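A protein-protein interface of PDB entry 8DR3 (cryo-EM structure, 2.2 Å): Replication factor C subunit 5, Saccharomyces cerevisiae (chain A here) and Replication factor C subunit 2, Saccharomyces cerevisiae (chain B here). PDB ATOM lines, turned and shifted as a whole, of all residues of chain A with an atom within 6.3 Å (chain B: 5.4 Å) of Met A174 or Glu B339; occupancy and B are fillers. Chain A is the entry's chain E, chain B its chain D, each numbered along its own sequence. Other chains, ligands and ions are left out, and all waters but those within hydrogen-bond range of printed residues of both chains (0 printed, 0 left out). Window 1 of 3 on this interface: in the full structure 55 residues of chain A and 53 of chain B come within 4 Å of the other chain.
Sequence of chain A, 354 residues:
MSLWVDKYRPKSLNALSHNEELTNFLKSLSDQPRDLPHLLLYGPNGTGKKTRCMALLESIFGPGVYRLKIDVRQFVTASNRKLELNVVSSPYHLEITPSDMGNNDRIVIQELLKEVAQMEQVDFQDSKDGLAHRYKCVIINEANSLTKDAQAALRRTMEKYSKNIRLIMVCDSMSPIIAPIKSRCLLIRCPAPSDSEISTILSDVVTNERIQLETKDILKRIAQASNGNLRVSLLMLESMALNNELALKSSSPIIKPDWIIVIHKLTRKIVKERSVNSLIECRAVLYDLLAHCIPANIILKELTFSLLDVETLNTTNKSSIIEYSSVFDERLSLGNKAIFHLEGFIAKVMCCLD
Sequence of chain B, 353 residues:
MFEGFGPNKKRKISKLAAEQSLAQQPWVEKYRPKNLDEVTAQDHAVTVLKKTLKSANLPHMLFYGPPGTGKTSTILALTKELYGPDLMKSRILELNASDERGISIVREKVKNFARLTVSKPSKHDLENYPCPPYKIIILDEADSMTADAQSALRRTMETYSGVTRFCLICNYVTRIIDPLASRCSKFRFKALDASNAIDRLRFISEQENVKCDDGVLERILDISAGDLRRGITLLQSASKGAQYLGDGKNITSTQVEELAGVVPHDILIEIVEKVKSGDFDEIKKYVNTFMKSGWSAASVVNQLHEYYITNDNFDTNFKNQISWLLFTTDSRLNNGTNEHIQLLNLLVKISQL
The backbone carbonyl oxygen (O) of Thr B337 sits at hydrogen-bond distance from the side-chain hydroxyl (OG) of Ser A175. The side-chain carboxylate (OE2) of Glu B339 sits at hydrogen-bond distance from the side-chain hydroxyl (OG) of Ser A173, 2.9 Å away. N of Asn B338 lies within hydrogen-bond range of OD2 of Asp A329 (2.7 Å).
The backbone NH of Ala B297 is in hydrogen-bond range of the side-chain carboxylate of Glu B339. The backbone NH of His B340 lies within hydrogen-bond range of the side-chain amide oxygen of Asn B338, 3.2 Å away. OG of Ser A173 sits at hydrogen-bond distance from N of Ser A175 (3.3 Å). N of Ile B341 lies within hydrogen-bond range of OD1 of Asn B338 (3.1 Å). The backbone carbonyl oxygen (O) of Ser A173 is in hydrogen-bond range of the side-chain sulfur (SG) of Cys A171, 3.3 Å away.
Among the printed residues, pairs that only touch across the chains: Met A174 with Glu B339 (3.6 Å), Ser A175 with Leu B333 (3.996 Å), Ser A175 with Glu B339 (3.6 Å), Asp A329 with Thr B337 (3.1 Å) and Asp A329 with Gln B342 (3.6 Å).
Of chain A, only Ser A173 (2.9 Å), Met A174 (3.6 Å) and Ser A175 (3.6 Å) come within 4 Å of Glu B339. Of the printed residues of chain B, Ser A173 touches Glu B339. Printed residues of chain B within 4 Å of Ser A175: Leu B333, Thr B337 and Glu B339. Of the printed residues of chain A, Asn B338 touches Asp A329 (2.7 Å). Of the printed residues of chain A, Leu B333 touches Ser A175. Printed residues of chain A within 4 Å of Gln B342: Asp A329 (3.6 Å).
Along chain A the printed residues that touch a printed residue of chain B span positions 173 to 329. Among the printed residues, no Asp or Glu carboxylate lies within 4 Å of a Lys or Arg side-chain nitrogen of the other chain.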
ATOM      1  N   LEU A  40      -1.182 -26.243 -29.163  1.00  0.00           N
ATOM      2  CA  LEU A  40      -2.378 -25.951 -28.375  1.00  0.00           C
ATOM      3  C   LEU A  40      -2.932 -24.620 -28.875  1.00  0.00           C
ATOM      4  O   LEU A  40      -2.411 -23.555 -28.533  1.00  0.00           O
ATOM      5  CB  LEU A  40      -2.062 -25.907 -26.883  1.00  0.00           C
ATOM      6  CG  LEU A  40      -3.188 -25.442 -25.954  1.00  0.00           C
ATOM      7  CD1 LEU A  40      -4.496 -26.146 -26.279  1.00  0.00           C
ATOM      8  CD2 LEU A  40      -2.808 -25.667 -24.498  1.00  0.00           C
ATOM      9  N   TYR A  42      -5.617 -21.898 -28.715  1.00  0.00           N
ATOM     10  CA  TYR A  42      -6.617 -21.377 -27.796  1.00  0.00           C
ATOM     11  C   TYR A  42      -7.189 -20.076 -28.337  1.00  0.00           C
ATOM     12  O   TYR A  42      -6.456 -19.234 -28.871  1.00  0.00           O
ATOM     13  CB  TYR A  42      -6.030 -21.157 -26.395  1.00  0.00           C
ATOM     14  CG  TYR A  42      -4.939 -20.113 -26.312  1.00  0.00           C
ATOM     15  CD1 TYR A  42      -3.633 -20.413 -26.676  1.00  0.00           C
ATOM     16  CD2 TYR A  42      -5.212 -18.833 -25.851  1.00  0.00           C
ATOM     17  CE1 TYR A  42      -2.632 -19.463 -26.593  1.00  0.00           C
ATOM     18  CE2 TYR A  42      -4.219 -17.876 -25.766  1.00  0.00           C
ATOM     19  CZ  TYR A  42      -2.932 -18.197 -26.136  1.00  0.00           C
ATOM     20  OH  TYR A  42      -1.941 -17.247 -26.051  1.00  0.00           O
ATOM     21  N   ASN A 144     -10.144 -28.594 -23.196  1.00  0.00           N
ATOM     22  CA  ASN A 144     -10.356 -27.981 -21.891  1.00  0.00           C
ATOM     23  C   ASN A 144     -11.439 -28.680 -21.079  1.00  0.00           C
ATOM     24  O   ASN A 144     -11.582 -28.381 -19.890  1.00  0.00           O
ATOM     25  CB  ASN A 144     -10.707 -26.501 -22.060  1.00  0.00           C
ATOM     26  CG  ASN A 144     -12.006 -26.286 -22.810  1.00  0.00           C
ATOM     27  OD1 ASN A 144     -12.606 -27.230 -23.324  1.00  0.00           O
ATOM     28  ND2 ASN A 144     -12.447 -25.037 -22.880  1.00  0.00           N
ATOM     29  N   CYS A 171      -8.900 -25.326 -27.922  1.00  0.00           N
ATOM     30  CA  CYS A 171      -9.666 -24.957 -26.739  1.00  0.00           C
ATOM     31  C   CYS A 171     -10.152 -23.516 -26.832  1.00  0.00           C
ATOM     32  O   CYS A 171      -9.521 -22.654 -27.460  1.00  0.00           O
ATOM     33  CB  CYS A 171      -8.841 -25.152 -25.460  1.00  0.00           C
ATOM     34  SG  CYS A 171      -7.645 -23.843 -25.125  1.00  0.00           S
ATOM     35  N   ASP A 172     -11.297 -23.271 -26.190  1.00  0.00           N
ATOM     36  CA  ASP A 172     -11.827 -21.922 -26.063  1.00  0.00           C
ATOM     37  C   ASP A 172     -11.236 -21.175 -24.877  1.00  0.00           C
ATOM     38  O   ASP A 172     -11.386 -19.952 -24.794  1.00  0.00           O
ATOM     39  CB  ASP A 172     -13.352 -21.965 -25.936  1.00  0.00           C
ATOM     40  CG  ASP A 172     -13.813 -22.690 -24.686  1.00  0.00           C
ATOM     41  OD1 ASP A 172     -14.319 -23.825 -24.811  1.00  0.00           O
ATOM     42  OD2 ASP A 172     -13.671 -22.128 -23.581  1.00  0.00           O
ATOM     43  N   SER A 173     -10.572 -21.879 -23.963  1.00  0.00           N
ATOM     44  CA  SER A 173      -9.965 -21.259 -22.797  1.00  0.00           C
ATOM     45  C   SER A 173      -8.929 -22.214 -22.224  1.00  0.00           C
ATOM     46  O   SER A 173      -9.147 -23.428 -22.197  1.00  0.00           O
ATOM     47  CB  SER A 173     -11.017 -20.913 -21.736  1.00  0.00           C
ATOM     48  OG  SER A 173     -10.411 -20.651 -20.483  1.00  0.00           O
ATOM     49  N   MET A 174      -7.808 -21.661 -21.771  1.00  0.00           N
ATOM     50  CA  MET A 174      -6.725 -22.449 -21.198  1.00  0.00           C
ATOM     51  C   MET A 174      -6.820 -22.586 -19.684  1.00  0.00           C
ATOM     52  O   MET A 174      -6.004 -23.298 -19.091  1.00  0.00           O
ATOM     53  CB  MET A 174      -5.375 -21.826 -21.564  1.00  0.00           C
ATOM     54  CG  MET A 174      -5.075 -21.823 -23.052  1.00  0.00           C
ATOM     55  SD  MET A 174      -3.306 -21.845 -23.390  1.00  0.00           S
ATOM     56  CE  MET A 174      -2.895 -20.127 -23.092  1.00  0.00           C
ATOM     57  N   SER A 175      -7.787 -21.929 -19.046  1.00  0.00           N
ATOM     58  CA  SER A 175      -7.867 -21.982 -17.589  1.00  0.00           C
ATOM     59  C   SER A 175      -7.999 -23.403 -17.050  1.00  0.00           C
ATOM     60  O   SER A 175      -7.349 -23.708 -16.035  1.00  0.00           O
ATOM     61  CB  SER A 175      -9.020 -21.095 -17.099  1.00  0.00           C
ATOM     62  OG  SER A 175     -10.243 -21.805 -17.029  1.00  0.00           O
ATOM     63  N   PRO A 176      -8.794 -24.300 -17.641  1.00  0.00           N
ATOM     64  CA  PRO A 176      -8.913 -25.657 -17.090  1.00  0.00           C
ATOM     65  C   PRO A 176      -7.782 -26.600 -17.477  1.00  0.00           C
ATOM     66  O   PRO A 176      -7.778 -27.746 -17.012  1.00  0.00           O
ATOM     67  CB  PRO A 176     -10.256 -26.150 -17.667  1.00  0.00           C
ATOM     68  CG  PRO A 176     -10.849 -24.978 -18.423  1.00  0.00           C
ATOM     69  CD  PRO A 176      -9.700 -24.111 -18.784  1.00  0.00           C
ATOM     70  N   ILE A 177      -6.831 -26.170 -18.302  1.00  0.00           N
ATOM     71  CA  ILE A 177      -5.713 -27.024 -18.693  1.00  0.00           C
ATOM     72  C   ILE A 177      -4.650 -26.978 -17.603  1.00  0.00           C
ATOM     73  O   ILE A 177      -4.226 -25.897 -17.178  1.00  0.00           O
ATOM     74  CB  ILE A 177      -5.135 -26.582 -20.048  1.00  0.00           C
ATOM     75  CG1 ILE A 177      -6.225 -26.560 -21.126  1.00  0.00           C
ATOM     76  CG2 ILE A 177      -3.987 -27.495 -20.462  1.00  0.00           C
ATOM     77  CD1 ILE A 177      -6.782 -27.923 -21.478  1.00  0.00           C
ATOM     78  N   ILE A 178      -4.214 -28.154 -17.148  1.00  0.00           N
ATOM     79  CA  ILE A 178      -3.235 -28.216 -16.068  1.00  0.00           C
ATOM     80  C   ILE A 178      -1.887 -27.696 -16.556  1.00  0.00           C
ATOM     81  O   ILE A 178      -1.573 -27.728 -17.754  1.00  0.00           O
ATOM     82  CB  ILE A 178      -3.115 -29.650 -15.517  1.00  0.00           C
ATOM     83  CG1 ILE A 178      -2.612 -30.615 -16.596  1.00  0.00           C
ATOM     84  CG2 ILE A 178      -4.455 -30.118 -14.970  1.00  0.00           C
ATOM     85  CD1 ILE A 178      -2.330 -32.011 -16.080  1.00  0.00           C
ATOM     86  N   LYS A 182       0.216 -27.551 -20.479  1.00  0.00           N
ATOM     87  CA  LYS A 182       0.567 -26.290 -21.121  1.00  0.00           C
ATOM     88  C   LYS A 182       2.071 -26.192 -21.336  1.00  0.00           C
ATOM     89  O   LYS A 182       2.529 -25.719 -22.383  1.00  0.00           O
ATOM     90  CB  LYS A 182       0.067 -25.115 -20.280  1.00  0.00           C
ATOM     91  CG  LYS A 182      -1.385 -24.748 -20.534  1.00  0.00           C
ATOM     92  CD  LYS A 182      -2.022 -24.093 -19.316  1.00  0.00           C
ATOM     93  CE  LYS A 182      -1.310 -22.806 -18.926  1.00  0.00           C
ATOM     94  NZ  LYS A 182      -1.277 -21.818 -20.039  1.00  0.00           N
ATOM     95  N   LEU A 187       1.872 -22.916 -27.479  1.00  0.00           N
ATOM     96  CA  LEU A 187       0.607 -22.200 -27.364  1.00  0.00           C
ATOM     97  C   LEU A 187       0.431 -21.243 -28.536  1.00  0.00           C
ATOM     98  O   LEU A 187       1.348 -20.491 -28.879  1.00  0.00           O
ATOM     99  CB  LEU A 187       0.550 -21.435 -26.043  1.00  0.00           C
ATOM    100  CG  LEU A 187       1.031 -22.196 -24.804  1.00  0.00           C
ATOM    101  CD1 LEU A 187       0.944 -21.319 -23.566  1.00  0.00           C
ATOM    102  CD2 LEU A 187       0.232 -23.476 -24.612  1.00  0.00           C
ATOM    103  N   ASP A 329     -19.568 -19.108 -10.431  1.00  0.00           N
ATOM    104  CA  ASP A 329     -18.847 -19.767 -11.512  1.00  0.00           C
ATOM    105  C   ASP A 329     -17.777 -20.694 -10.954  1.00  0.00           C
ATOM    106  O   ASP A 329     -17.607 -21.823 -11.433  1.00  0.00           O
ATOM    107  CB  ASP A 329     -18.232 -18.720 -12.442  1.00  0.00           C
ATOM    108  CG  ASP A 329     -17.396 -19.337 -13.543  1.00  0.00           C
ATOM    109  OD1 ASP A 329     -17.944 -20.131 -14.336  1.00  0.00           O
ATOM    110  OD2 ASP A 329     -16.193 -19.021 -13.623  1.00  0.00           O
ATOM    111  N   MET B 291     -11.577  -9.172 -24.554  1.00  0.00           N
ATOM    112  CA  MET B 291     -11.637 -10.631 -24.571  1.00  0.00           C
ATOM    113  C   MET B 291     -11.660 -11.196 -25.985  1.00  0.00           C
ATOM    114  O   MET B 291     -11.309 -12.364 -26.178  1.00  0.00           O
ATOM    115  CB  MET B 291     -12.868 -11.123 -23.805  1.00  0.00           C
ATOM    116  CG  MET B 291     -12.837 -10.855 -22.306  1.00  0.00           C
ATOM    117  SD  MET B 291     -11.354 -11.478 -21.492  1.00  0.00           S
ATOM    118  CE  MET B 291     -11.703 -13.233 -21.447  1.00  0.00           C
ATOM    119  N   TRP B 295      -6.501 -13.060 -25.304  1.00  0.00           N
ATOM    120  CA  TRP B 295      -5.422 -13.039 -24.324  1.00  0.00           C
ATOM    121  C   TRP B 295      -5.752 -13.949 -23.148  1.00  0.00           C
ATOM    122  O   TRP B 295      -6.891 -13.997 -22.676  1.00  0.00           O
ATOM    123  CB  TRP B 295      -5.182 -11.614 -23.823  1.00  0.00           C
ATOM    124  CG  TRP B 295      -4.800 -10.644 -24.895  1.00  0.00           C
ATOM    125  CD1 TRP B 295      -5.548  -9.604 -25.362  1.00  0.00           C
ATOM    126  CD2 TRP B 295      -3.572 -10.618 -25.629  1.00  0.00           C
ATOM    127  NE1 TRP B 295      -4.863  -8.932 -26.344  1.00  0.00           N
ATOM    128  CE2 TRP B 295      -3.646  -9.535 -26.529  1.00  0.00           C
ATOM    129  CE3 TRP B 295      -2.417 -11.406 -25.617  1.00  0.00           C
ATOM    130  CZ2 TRP B 295      -2.612  -9.221 -27.406  1.00  0.00           C
ATOM    131  CZ3 TRP B 295      -1.392 -11.091 -26.488  1.00  0.00           C
ATOM    132  CH2 TRP B 295      -1.495 -10.009 -27.370  1.00  0.00           C
ATOM    133  N   SER B 296      -4.744 -14.677 -22.676  1.00  0.00           N
ATOM    134  CA  SER B 296      -4.920 -15.530 -21.511  1.00  0.00           C
ATOM    135  C   SER B 296      -5.122 -14.685 -20.259  1.00  0.00           C
ATOM    136  O   SER B 296      -4.409 -13.703 -20.030  1.00  0.00           O
ATOM    137  CB  SER B 296      -3.708 -16.447 -21.337  1.00  0.00           C
ATOM    138  OG  SER B 296      -3.551 -16.834 -19.985  1.00  0.00           O
ATOM    139  N   ALA B 297      -6.103 -15.074 -19.441  1.00  0.00           N
ATOM    140  CA  ALA B 297      -6.403 -14.311 -18.234  1.00  0.00           C
ATOM    141  C   ALA B 297      -5.242 -14.351 -17.250  1.00  0.00           C
ATOM    142  O   ALA B 297      -4.954 -13.353 -16.578  1.00  0.00           O
ATOM    143  CB  ALA B 297      -7.675 -14.845 -17.579  1.00  0.00           C
ATOM    144  N   LEU B 333      -8.965 -18.533 -10.796  1.00  0.00           N
ATOM    145  CA  LEU B 333      -8.635 -18.937 -12.159  1.00  0.00           C
ATOM    146  C   LEU B 333      -7.977 -20.310 -12.189  1.00  0.00           C
ATOM    147  O   LEU B 333      -8.162 -21.066 -13.149  1.00  0.00           O
ATOM    148  CB  LEU B 333      -7.717 -17.900 -12.807  1.00  0.00           C
ATOM    149  CG  LEU B 333      -8.399 -16.646 -13.361  1.00  0.00           C
ATOM    150  CD1 LEU B 333      -7.370 -15.561 -13.636  1.00  0.00           C
ATOM    151  CD2 LEU B 333      -9.192 -16.965 -14.618  1.00  0.00           C
ATOM    152  N   THR B 337     -12.069 -21.520 -14.154  1.00  0.00           N
ATOM    153  CA  THR B 337     -13.258 -20.683 -14.196  1.00  0.00           C
ATOM    154  C   THR B 337     -13.315 -19.889 -15.498  1.00  0.00           C
ATOM    155  O   THR B 337     -12.355 -19.831 -16.269  1.00  0.00           O
ATOM    156  CB  THR B 337     -13.287 -19.733 -12.994  1.00  0.00           C
ATOM    157  OG1 THR B 337     -11.972 -19.212 -12.758  1.00  0.00           O
ATOM    158  CG2 THR B 337     -13.775 -20.458 -11.752  1.00  0.00           C
ATOM    159  N   ASN B 338     -14.470 -19.272 -15.736  1.00  0.00           N
ATOM    160  CA  ASN B 338     -14.652 -18.423 -16.908  1.00  0.00           C
ATOM    161  C   ASN B 338     -13.745 -17.202 -16.803  1.00  0.00           C
ATOM    162  O   ASN B 338     -13.845 -16.426 -15.848  1.00  0.00           O
ATOM    163  CB  ASN B 338     -16.114 -17.999 -17.029  1.00  0.00           C
ATOM    164  CG  ASN B 338     -16.402 -17.259 -18.319  1.00  0.00           C
ATOM    165  OD1 ASN B 338     -16.362 -16.030 -18.365  1.00  0.00           O
ATOM    166  ND2 ASN B 338     -16.696 -18.005 -19.376  1.00  0.00           N
ATOM    167  N   GLU B 339     -12.864 -17.029 -17.790  1.00  0.00           N
ATOM    168  CA  GLU B 339     -11.884 -15.947 -17.728  1.00  0.00           C
ATOM    169  C   GLU B 339     -12.556 -14.578 -17.770  1.00  0.00           C
ATOM    170  O   GLU B 339     -12.153 -13.659 -17.049  1.00  0.00           O
ATOM    171  CB  GLU B 339     -10.884 -16.089 -18.875  1.00  0.00           C
ATOM    172  CG  GLU B 339      -9.887 -17.223 -18.685  1.00  0.00           C
ATOM    173  CD  GLU B 339      -8.968 -17.404 -19.877  1.00  0.00           C
ATOM    174  OE1 GLU B 339      -8.755 -16.424 -20.623  1.00  0.00           O
ATOM    175  OE2 GLU B 339      -8.458 -18.527 -20.071  1.00  0.00           O
ATOM    176  N   HIS B 340     -13.576 -14.424 -18.614  1.00  0.00           N
ATOM    177  CA  HIS B 340     -14.228 -13.127 -18.779  1.00  0.00           C
ATOM    178  C   HIS B 340     -14.793 -12.621 -17.454  1.00  0.00           C
ATOM    179  O   HIS B 340     -14.535 -11.480 -17.048  1.00  0.00           O
ATOM    180  CB  HIS B 340     -15.331 -13.250 -19.833  1.00  0.00           C
ATOM    181  CG  HIS B 340     -15.855 -11.940 -20.332  1.00  0.00           C
ATOM    182  ND1 HIS B 340     -15.677 -10.754 -19.654  1.00  0.00           N
ATOM    183  CD2 HIS B 340     -16.556 -11.631 -21.448  1.00  0.00           C
ATOM    184  CE1 HIS B 340     -16.247  -9.772 -20.330  1.00  0.00           C
ATOM    185  NE2 HIS B 340     -16.786 -10.278 -21.424  1.00  0.00           N
ATOM    186  N   ILE B 341     -15.563 -13.465 -16.764  1.00  0.00           N
ATOM    187  CA  ILE B 341     -16.216 -13.045 -15.526  1.00  0.00           C
ATOM    188  C   ILE B 341     -15.176 -12.688 -14.472  1.00  0.00           C
ATOM    189  O   ILE B 341     -15.274 -11.651 -13.803  1.00  0.00           O
ATOM    190  CB  ILE B 341     -17.168 -14.148 -15.028  1.00  0.00           C
ATOM    191  CG1 ILE B 341     -18.370 -14.278 -15.966  1.00  0.00           C
ATOM    192  CG2 ILE B 341     -17.631 -13.856 -13.606  1.00  0.00           C
ATOM    193  CD1 ILE B 341     -19.064 -15.620 -15.885  1.00  0.00           C
ATOM    194  N   GLN B 342     -14.168 -13.546 -14.304  1.00  0.00           N
ATOM    195  CA  GLN B 342     -13.158 -13.307 -13.280  1.00  0.00           C
ATOM    196  C   GLN B 342     -12.381 -12.027 -13.560  1.00  0.00           C
ATOM    197  O   GLN B 342     -12.123 -11.235 -12.646  1.00  0.00           O
ATOM    198  CB  GLN B 342     -12.210 -14.503 -13.189  1.00  0.00           C
ATOM    199  CG  GLN B 342     -12.902 -15.823 -12.871  1.00  0.00           C
ATOM    200  CD  GLN B 342     -13.577 -15.821 -11.514  1.00  0.00           C
ATOM    201  OE1 GLN B 342     -13.236 -15.030 -10.638  1.00  0.00           O
ATOM    202  NE2 GLN B 342     -14.544 -16.713 -11.336  1.00  0.00           N
ATOM    203  N   LEU B 343     -11.997 -11.806 -14.821  1.00  0.00           N
ATOM    204  CA  LEU B 343     -11.250 -10.602 -15.161  1.00  0.00           C
ATOM    205  C   LEU B 343     -12.087  -9.350 -14.932  1.00  0.00           C
ATOM    206  O   LEU B 343     -11.589  -8.351 -14.395  1.00  0.00           O
ATOM    207  CB  LEU B 343     -10.773 -10.671 -16.612  1.00  0.00           C
ATOM    208  CG  LEU B 343      -9.942  -9.480 -17.102  1.00  0.00           C
ATOM    209  CD1 LEU B 343      -8.708  -9.281 -16.236  1.00  0.00           C
ATOM    210  CD2 LEU B 343      -9.550  -9.664 -18.559  1.00  0.00           C
ATOM    211  N   LEU B 344     -13.360  -9.379 -15.336  1.00  0.00           N
ATOM    212  CA  LEU B 344     -14.216  -8.218 -15.115  1.00  0.00           C
ATOM    213  C   LEU B 344     -14.379  -7.937 -13.627  1.00  0.00           C
ATOM    214  O   LEU B 344     -14.316  -6.779 -13.194  1.00  0.00           O
ATOM    215  CB  LEU B 344     -15.577  -8.434 -15.777  1.00  0.00           C
ATOM    216  CG  LEU B 344     -16.591  -7.296 -15.627  1.00  0.00           C
ATOM    217  CD1 LEU B 344     -16.014  -5.978 -16.127  1.00  0.00           C
ATOM    218  CD2 LEU B 344     -17.876  -7.630 -16.367  1.00  0.00           C
